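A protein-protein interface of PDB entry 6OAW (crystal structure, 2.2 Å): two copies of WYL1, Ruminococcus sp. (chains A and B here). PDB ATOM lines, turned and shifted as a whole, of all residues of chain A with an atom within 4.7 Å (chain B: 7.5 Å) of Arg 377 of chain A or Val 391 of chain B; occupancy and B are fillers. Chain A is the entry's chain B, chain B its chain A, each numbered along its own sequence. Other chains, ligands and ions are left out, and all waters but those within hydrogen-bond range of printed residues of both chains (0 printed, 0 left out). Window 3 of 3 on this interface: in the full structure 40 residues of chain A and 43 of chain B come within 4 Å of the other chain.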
ATOM      1  N   PHE A 373     -24.052 -30.849 -21.820  1.00  0.00           N
ATOM      2  CA  PHE A 373     -23.737 -30.100 -23.057  1.00  0.00           C
ATOM      3  C   PHE A 373     -22.378 -29.390 -22.918  1.00  0.00           C
ATOM      4  O   PHE A 373     -21.531 -29.547 -23.804  1.00  0.00           O
ATOM      5  CB  PHE A 373     -24.812 -29.083 -23.385  1.00  0.00           C
ATOM      6  CG  PHE A 373     -24.445 -28.325 -24.627  1.00  0.00           C
ATOM      7  CD1 PHE A 373     -24.587 -28.928 -25.855  1.00  0.00           C
ATOM      8  CD2 PHE A 373     -23.972 -27.026 -24.556  1.00  0.00           C
ATOM      9  CE1 PHE A 373     -24.246 -28.256 -27.006  1.00  0.00           C
ATOM     10  CE2 PHE A 373     -23.619 -26.367 -25.716  1.00  0.00           C
ATOM     11  CZ  PHE A 373     -23.743 -26.985 -26.933  1.00  0.00           C
ATOM     12  N   GLU A 374     -22.170 -28.678 -21.814  1.00  0.00           N
ATOM     13  CA  GLU A 374     -20.983 -27.818 -21.597  1.00  0.00           C
ATOM     14  C   GLU A 374     -19.714 -28.692 -21.433  1.00  0.00           C
ATOM     15  O   GLU A 374     -18.667 -28.327 -22.000  1.00  0.00           O
ATOM     16  CB  GLU A 374     -21.223 -26.893 -20.406  1.00  0.00           C
ATOM     17  CG  GLU A 374     -22.338 -25.866 -20.638  1.00  0.00           C
ATOM     18  CD  GLU A 374     -22.868 -25.192 -19.387  1.00  0.00           C
ATOM     19  OE1 GLU A 374     -23.986 -24.611 -19.448  1.00  0.00           O
ATOM     20  OE2 GLU A 374     -22.127 -25.185 -18.382  1.00  0.00           O
ATOM     21  N   GLU A 375     -19.809 -29.827 -20.729  1.00  0.00           N
ATOM     22  CA  GLU A 375     -18.661 -30.766 -20.569  1.00  0.00           C
ATOM     23  C   GLU A 375     -18.312 -31.378 -21.928  1.00  0.00           C
ATOM     24  O   GLU A 375     -17.141 -31.435 -22.242  1.00  0.00           O
ATOM     25  CB  GLU A 375     -18.928 -31.907 -19.586  1.00  0.00           C
ATOM     26  CG  GLU A 375     -18.814 -31.476 -18.144  1.00  0.00           C
ATOM     27  CD  GLU A 375     -19.273 -32.553 -17.180  1.00  0.00           C
ATOM     28  OE1 GLU A 375     -20.183 -32.252 -16.343  1.00  0.00           O
ATOM     29  OE2 GLU A 375     -18.761 -33.713 -17.336  1.00  0.00           O
ATOM     30  N   MET A 376     -19.303 -31.831 -22.685  1.00  0.00           N
ATOM     31  CA  MET A 376     -19.050 -32.453 -24.006  1.00  0.00           C
ATOM     32  C   MET A 376     -18.434 -31.403 -24.928  1.00  0.00           C
ATOM     33  O   MET A 376     -17.444 -31.750 -25.589  1.00  0.00           O
ATOM     34  CB  MET A 376     -20.326 -33.014 -24.621  1.00  0.00           C
ATOM     35  CG  MET A 376     -20.907 -34.210 -23.870  1.00  0.00           C
ATOM     36  SD  MET A 376     -19.616 -35.691 -23.570  1.00  0.00           S
ATOM     37  CE  MET A 376     -18.794 -35.267 -21.826  1.00  0.00           C
ATOM     38  N   ARG A 377     -18.961 -30.161 -24.932  1.00  0.00           N
ATOM     39  CA  ARG A 377     -18.433 -29.099 -25.818  1.00  0.00           C
ATOM     40  C   ARG A 377     -16.943 -28.868 -25.489  1.00  0.00           C
ATOM     41  O   ARG A 377     -16.142 -28.799 -26.433  1.00  0.00           O
ATOM     42  CB  ARG A 377     -19.219 -27.794 -25.720  1.00  0.00           C
ATOM     43  CG  ARG A 377     -18.743 -26.756 -26.732  1.00  0.00           C
ATOM     44  CD  ARG A 377     -19.449 -25.454 -26.510  1.00  0.00           C
ATOM     45  NE  ARG A 377     -19.093 -24.490 -27.540  1.00  0.00           N
ATOM     46  CZ  ARG A 377     -19.002 -23.180 -27.340  1.00  0.00           C
ATOM     47  NH1 ARG A 377     -19.268 -22.673 -26.147  1.00  0.00           N
ATOM     48  NH2 ARG A 377     -18.657 -22.381 -28.333  1.00  0.00           N
ATOM     49  N   THR A 378     -16.602 -28.734 -24.208  1.00  0.00           N
ATOM     50  CA  THR A 378     -15.212 -28.567 -23.714  1.00  0.00           C
ATOM     51  C   THR A 378     -14.358 -29.773 -24.157  1.00  0.00           C
ATOM     52  O   THR A 378     -13.309 -29.549 -24.783  1.00  0.00           O
ATOM     53  CB  THR A 378     -15.220 -28.418 -22.187  1.00  0.00           C
ATOM     54  OG1 THR A 378     -15.906 -27.191 -21.958  1.00  0.00           O
ATOM     55  CG2 THR A 378     -13.835 -28.381 -21.561  1.00  0.00           C
ATOM     56  N   LEU A 379     -14.800 -31.006 -23.863  1.00  0.00           N
ATOM     57  CA  LEU A 379     -14.023 -32.221 -24.223  1.00  0.00           C
ATOM     58  C   LEU A 379     -13.699 -32.182 -25.720  1.00  0.00           C
ATOM     59  O   LEU A 379     -12.506 -32.343 -26.091  1.00  0.00           O
ATOM     60  CB  LEU A 379     -14.818 -33.476 -23.864  1.00  0.00           C
ATOM     61  CG  LEU A 379     -14.238 -34.807 -24.355  1.00  0.00           C
ATOM     62  CD1 LEU A 379     -12.897 -35.116 -23.672  1.00  0.00           C
ATOM     63  CD2 LEU A 379     -15.251 -35.934 -24.099  1.00  0.00           C
ATOM     64  N   TYR A 380     -14.708 -31.929 -26.547  1.00  0.00           N
ATOM     65  CA  TYR A 380     -14.575 -32.017 -28.020  1.00  0.00           C
ATOM     66  C   TYR A 380     -13.777 -30.826 -28.533  1.00  0.00           C
ATOM     67  O   TYR A 380     -12.924 -31.067 -29.398  1.00  0.00           O
ATOM     68  CB  TYR A 380     -15.937 -32.175 -28.698  1.00  0.00           C
ATOM     69  CG  TYR A 380     -16.305 -33.624 -28.771  1.00  0.00           C
ATOM     70  CD1 TYR A 380     -15.816 -34.419 -29.790  1.00  0.00           C
ATOM     71  CD2 TYR A 380     -16.978 -34.233 -27.733  1.00  0.00           C
ATOM     72  CE1 TYR A 380     -16.028 -35.784 -29.809  1.00  0.00           C
ATOM     73  CE2 TYR A 380     -17.191 -35.600 -27.736  1.00  0.00           C
ATOM     74  CZ  TYR A 380     -16.727 -36.380 -28.787  1.00  0.00           C
ATOM     75  OH  TYR A 380     -16.947 -37.731 -28.830  1.00  0.00           O
ATOM     76  N   VAL A 381     -14.028 -29.594 -28.058  1.00  0.00           N
ATOM     77  CA  VAL A 381     -13.338 -28.419 -28.655  1.00  0.00           C
ATOM     78  C   VAL A 381     -11.853 -28.544 -28.280  1.00  0.00           C
ATOM     79  O   VAL A 381     -11.033 -28.352 -29.155  1.00  0.00           O
ATOM     80  CB  VAL A 381     -13.966 -27.074 -28.229  1.00  0.00           C
ATOM     81  CG1 VAL A 381     -13.048 -25.880 -28.537  1.00  0.00           C
ATOM     82  CG2 VAL A 381     -15.317 -26.874 -28.893  1.00  0.00           C
ATOM     83  N   GLU A 382     -11.530 -28.890 -27.023  1.00  0.00           N
ATOM     84  CA  GLU A 382     -10.120 -28.975 -26.565  1.00  0.00           C
ATOM     85  C   GLU A 382      -9.446 -30.196 -27.216  1.00  0.00           C
ATOM     86  O   GLU A 382      -8.250 -30.105 -27.533  1.00  0.00           O
ATOM     87  CB  GLU A 382     -10.038 -28.950 -25.037  1.00  0.00           C
ATOM     88  CG  GLU A 382     -10.518 -27.607 -24.466  1.00  0.00           C
ATOM     89  CD  GLU A 382     -10.354 -27.373 -22.976  1.00  0.00           C
ATOM     90  OE1 GLU A 382     -10.036 -28.339 -22.241  1.00  0.00           O
ATOM     91  OE2 GLU A 382     -10.521 -26.207 -22.556  1.00  0.00           O
ATOM     92  N   GLY B 383     -17.107 -33.650 -33.990  1.00  0.00           N
ATOM     93  CA  GLY B 383     -17.812 -33.559 -32.699  1.00  0.00           C
ATOM     94  C   GLY B 383     -17.860 -32.120 -32.239  1.00  0.00           C
ATOM     95  O   GLY B 383     -18.989 -31.642 -31.924  1.00  0.00           O
ATOM     96  N   ALA B 384     -16.703 -31.444 -32.274  1.00  0.00           N
ATOM     97  CA  ALA B 384     -16.544 -30.035 -31.861  1.00  0.00           C
ATOM     98  C   ALA B 384     -17.488 -29.167 -32.698  1.00  0.00           C
ATOM     99  O   ALA B 384     -18.212 -28.317 -32.122  1.00  0.00           O
ATOM    100  CB  ALA B 384     -15.094 -29.606 -32.014  1.00  0.00           C
ATOM    101  N   ASP B 385     -17.505 -29.418 -34.011  1.00  0.00           N
ATOM    102  CA  ASP B 385     -18.344 -28.655 -34.956  1.00  0.00           C
ATOM    103  C   ASP B 385     -19.809 -28.865 -34.545  1.00  0.00           C
ATOM    104  O   ASP B 385     -20.559 -27.872 -34.522  1.00  0.00           O
ATOM    105  CB  ASP B 385     -17.993 -28.990 -36.416  1.00  0.00           C
ATOM    106  CG  ASP B 385     -16.682 -28.401 -36.961  1.00  0.00           C
ATOM    107  OD1 ASP B 385     -16.103 -27.467 -36.316  1.00  0.00           O
ATOM    108  OD2 ASP B 385     -16.218 -28.890 -38.046  1.00  0.00           O
ATOM    109  N   ALA B 386     -20.205 -30.095 -34.183  1.00  0.00           N
ATOM    110  CA  ALA B 386     -21.604 -30.410 -33.814  1.00  0.00           C
ATOM    111  C   ALA B 386     -21.973 -29.645 -32.537  1.00  0.00           C
ATOM    112  O   ALA B 386     -23.017 -28.951 -32.535  1.00  0.00           O
ATOM    113  CB  ALA B 386     -21.799 -31.893 -33.662  1.00  0.00           C
ATOM    114  N   TYR B 387     -21.142 -29.709 -31.506  1.00  0.00           N
ATOM    115  CA  TYR B 387     -21.421 -29.024 -30.211  1.00  0.00           C
ATOM    116  C   TYR B 387     -21.402 -27.496 -30.394  1.00  0.00           C
ATOM    117  O   TYR B 387     -22.314 -26.846 -29.895  1.00  0.00           O
ATOM    118  CB  TYR B 387     -20.473 -29.512 -29.115  1.00  0.00           C
ATOM    119  CG  TYR B 387     -20.872 -30.854 -28.567  1.00  0.00           C
ATOM    120  CD1 TYR B 387     -21.866 -30.951 -27.609  1.00  0.00           C
ATOM    121  CD2 TYR B 387     -20.276 -32.019 -29.026  1.00  0.00           C
ATOM    122  CE1 TYR B 387     -22.298 -32.178 -27.144  1.00  0.00           C
ATOM    123  CE2 TYR B 387     -20.676 -33.262 -28.540  1.00  0.00           C
ATOM    124  CZ  TYR B 387     -21.667 -33.328 -27.575  1.00  0.00           C
ATOM    125  OH  TYR B 387     -22.063 -34.520 -27.089  1.00  0.00           O
ATOM    126  N   ASN B 388     -20.436 -26.948 -31.132  1.00  0.00           N
ATOM    127  CA  ASN B 388     -20.345 -25.486 -31.418  1.00  0.00           C
ATOM    128  C   ASN B 388     -21.594 -25.044 -32.171  1.00  0.00           C
ATOM    129  O   ASN B 388     -22.113 -23.987 -31.827  1.00  0.00           O
ATOM    130  CB  ASN B 388     -19.079 -25.079 -32.191  1.00  0.00           C
ATOM    131  CG  ASN B 388     -17.856 -25.018 -31.300  1.00  0.00           C
ATOM    132  OD1 ASN B 388     -17.981 -24.905 -30.076  1.00  0.00           O
ATOM    133  ND2 ASN B 388     -16.675 -25.104 -31.901  1.00  0.00           N
ATOM    134  N   ARG B 389     -22.052 -25.814 -33.159  1.00  0.00           N
ATOM    135  CA  ARG B 389     -23.237 -25.439 -33.974  1.00  0.00           C
ATOM    136  C   ARG B 389     -24.422 -25.165 -33.030  1.00  0.00           C
ATOM    137  O   ARG B 389     -25.171 -24.209 -33.305  1.00  0.00           O
ATOM    138  CB  ARG B 389     -23.528 -26.531 -34.997  1.00  0.00           C
ATOM    139  CG  ARG B 389     -24.628 -26.252 -36.010  1.00  0.00           C
ATOM    140  CD  ARG B 389     -24.790 -27.470 -36.926  1.00  0.00           C
ATOM    141  NE  ARG B 389     -23.611 -27.677 -37.789  1.00  0.00           N
ATOM    142  CZ  ARG B 389     -22.750 -28.712 -37.778  1.00  0.00           C
ATOM    143  NH1 ARG B 389     -22.886 -29.730 -36.941  1.00  0.00           N
ATOM    144  NH2 ARG B 389     -21.730 -28.710 -38.627  1.00  0.00           N
ATOM    145  N   GLU B 390     -24.583 -25.933 -31.940  1.00  0.00           N
ATOM    146  CA  GLU B 390     -25.770 -25.792 -31.043  1.00  0.00           C
ATOM    147  C   GLU B 390     -25.718 -24.496 -30.213  1.00  0.00           C
ATOM    148  O   GLU B 390     -26.744 -24.134 -29.638  1.00  0.00           O
ATOM    149  CB  GLU B 390     -25.936 -27.027 -30.153  1.00  0.00           C
ATOM    150  CG  GLU B 390     -26.382 -28.253 -30.948  1.00  0.00           C
ATOM    151  CD  GLU B 390     -27.539 -28.023 -31.915  1.00  0.00           C
ATOM    152  OE1 GLU B 390     -28.624 -27.598 -31.462  1.00  0.00           O
ATOM    153  OE2 GLU B 390     -27.335 -28.223 -33.123  1.00  0.00           O
ATOM    154  N   VAL B 391     -24.559 -23.844 -30.127  1.00  0.00           N
ATOM    155  CA  VAL B 391     -24.382 -22.544 -29.417  1.00  0.00           C
ATOM    156  C   VAL B 391     -24.743 -21.374 -30.370  1.00  0.00           C
ATOM    157  O   VAL B 391     -25.039 -20.321 -29.884  1.00  0.00           O
ATOM    158  CB  VAL B 391     -22.952 -22.448 -28.844  1.00  0.00           C
ATOM    159  CG1 VAL B 391     -22.641 -21.054 -28.308  1.00  0.00           C
ATOM    160  CG2 VAL B 391     -22.729 -23.509 -27.772  1.00  0.00           C
ATOM    161  N   GLU B 392     -24.783 -21.578 -31.688  1.00  0.00           N
ATOM    162  CA  GLU B 392     -25.189 -20.543 -32.679  1.00  0.00           C
ATOM    163  C   GLU B 392     -26.708 -20.334 -32.632  1.00  0.00           C
ATOM    164  O   GLU B 392     -27.428 -21.321 -32.607  1.00  0.00           O
ATOM    165  CB  GLU B 392     -24.714 -20.911 -34.085  1.00  0.00           C
ATOM    166  CG  GLU B 392     -23.201 -21.062 -34.130  1.00  0.00           C
ATOM    167  CD  GLU B 392     -22.613 -21.747 -35.349  1.00  0.00           C
ATOM    168  OE1 GLU B 392     -23.351 -21.946 -36.342  1.00  0.00           O
ATOM    169  OE2 GLU B 392     -21.406 -22.100 -35.283  1.00  0.00           O
ATOM    170  N   MET B 393     -27.150 -19.075 -32.585  1.00  0.00           N
ATOM    171  CA  MET B 393     -28.560 -18.652 -32.837  1.00  0.00           C
ATOM    172  C   MET B 393     -28.816 -18.603 -34.348  1.00  0.00           C
ATOM    173  O   MET B 393     -27.911 -18.644 -35.197  1.00  0.00           O
ATOM    174  OXT MET B 393     -29.980 -18.500 -34.723  1.00  0.00           O
ATOM    175  CB  MET B 393     -28.834 -17.257 -32.267  1.00  0.00           C
ATOM    176  CG  MET B 393     -28.483 -17.099 -30.815  1.00  0.00           C
ATOM    177  SD  MET B 393     -29.349 -18.487 -29.733  1.00  0.00           S
ATOM    178  CE  MET B 393     -30.823 -17.565 -28.791  1.00  0.00           C
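OD1 of Asn 388 of chain B is in hydrogen-bond range of NE of Arg 377 of chain A (2.8 Å).
O of Tyr 387 of chain B touches CZ of Phe 373 of chain A, at 3.3 Å.
CB of Glu 390 of chain B touches CE1 of Phe 373 of chain A (3.8 Å).
Phe 373 of chain A touches Val 391 of chain B (CE2 to CG2, 3.6 Å).
Tyr 387 of chain B touches Arg 377 of chain A.
Arg 377 of chain A touches Val 391 of chain B (CZ to CG2, 3.8 Å).
Tyr 380 of chain A touches Gly 383 of chain B.
Ala 384 of chain B touches Tyr 380 of chain A (CB to O, 3.7 Å).
CD2 of Tyr 380 of chain A touches CE2 of Tyr 387 of chain B, 3.9 Å away.
Val 381 of chain A touches Ala 384 of chain B (CA to CB, 3.97 Å).
Asn 388 of chain B touches Val 381 of chain A.
Of the printed residues of chain B, Phe 373 of chain A touches Tyr 387 (3.3 Å), Glu 390 (3.8 Å) and Val 391 (3.6 Å).
Glu 375 of chain A touches none of the printed residues of chain B.
Of the printed residues of chain B, Met 376 of chain A touches Tyr 387 (3.3 Å).
Of chain B, only Tyr 387 (3.9 Å), Asn 388 (2.8 Å) and Val 391 (3.8 Å) come within 4 Å of Arg 377 of chain A.
Of the printed residues of chain B, Tyr 380 of chain A touches Gly 383, Ala 384 and Tyr 387.
Printed residues of chain A within 4 Å of Tyr 387 of chain B: Phe 373, Met 376, Arg 377 and Tyr 380.
Printed residues of chain A within 4 Å of Asn 388 of chain B: Arg 377 (2.8 Å) and Val 381 (3.5 Å).
Of chain A, only Phe 373 and Arg 377 come within 4 Å of Val 391 of chain B.
Of the 10 printed residues of chain A, 5 touch a printed residue of chain B.
Hydrophobic or aromatic side chains of chain A that line the printed part of chain B: Phe 373, Met 376, Tyr 380 and Val 381.
Printed residues of chain B that touch a printed residue of chain A: Gly 383, Ala 384, Tyr 387, Asn 388, Glu 390 and Val 391.
Hydrophobic or aromatic side chains of chain B that line the printed part of chain A: Ala 384, Tyr 387 and Val 391.
Among the printed residues, no Asp or Glu carboxylate lies within 4 Å of a Lys or Arg side-chain nitrogen of the other chain.
No position is printed for both chains.
Of the 12 pairs that touch across the chains among the printed residues, none has its exchanged pair printed and touching as well.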
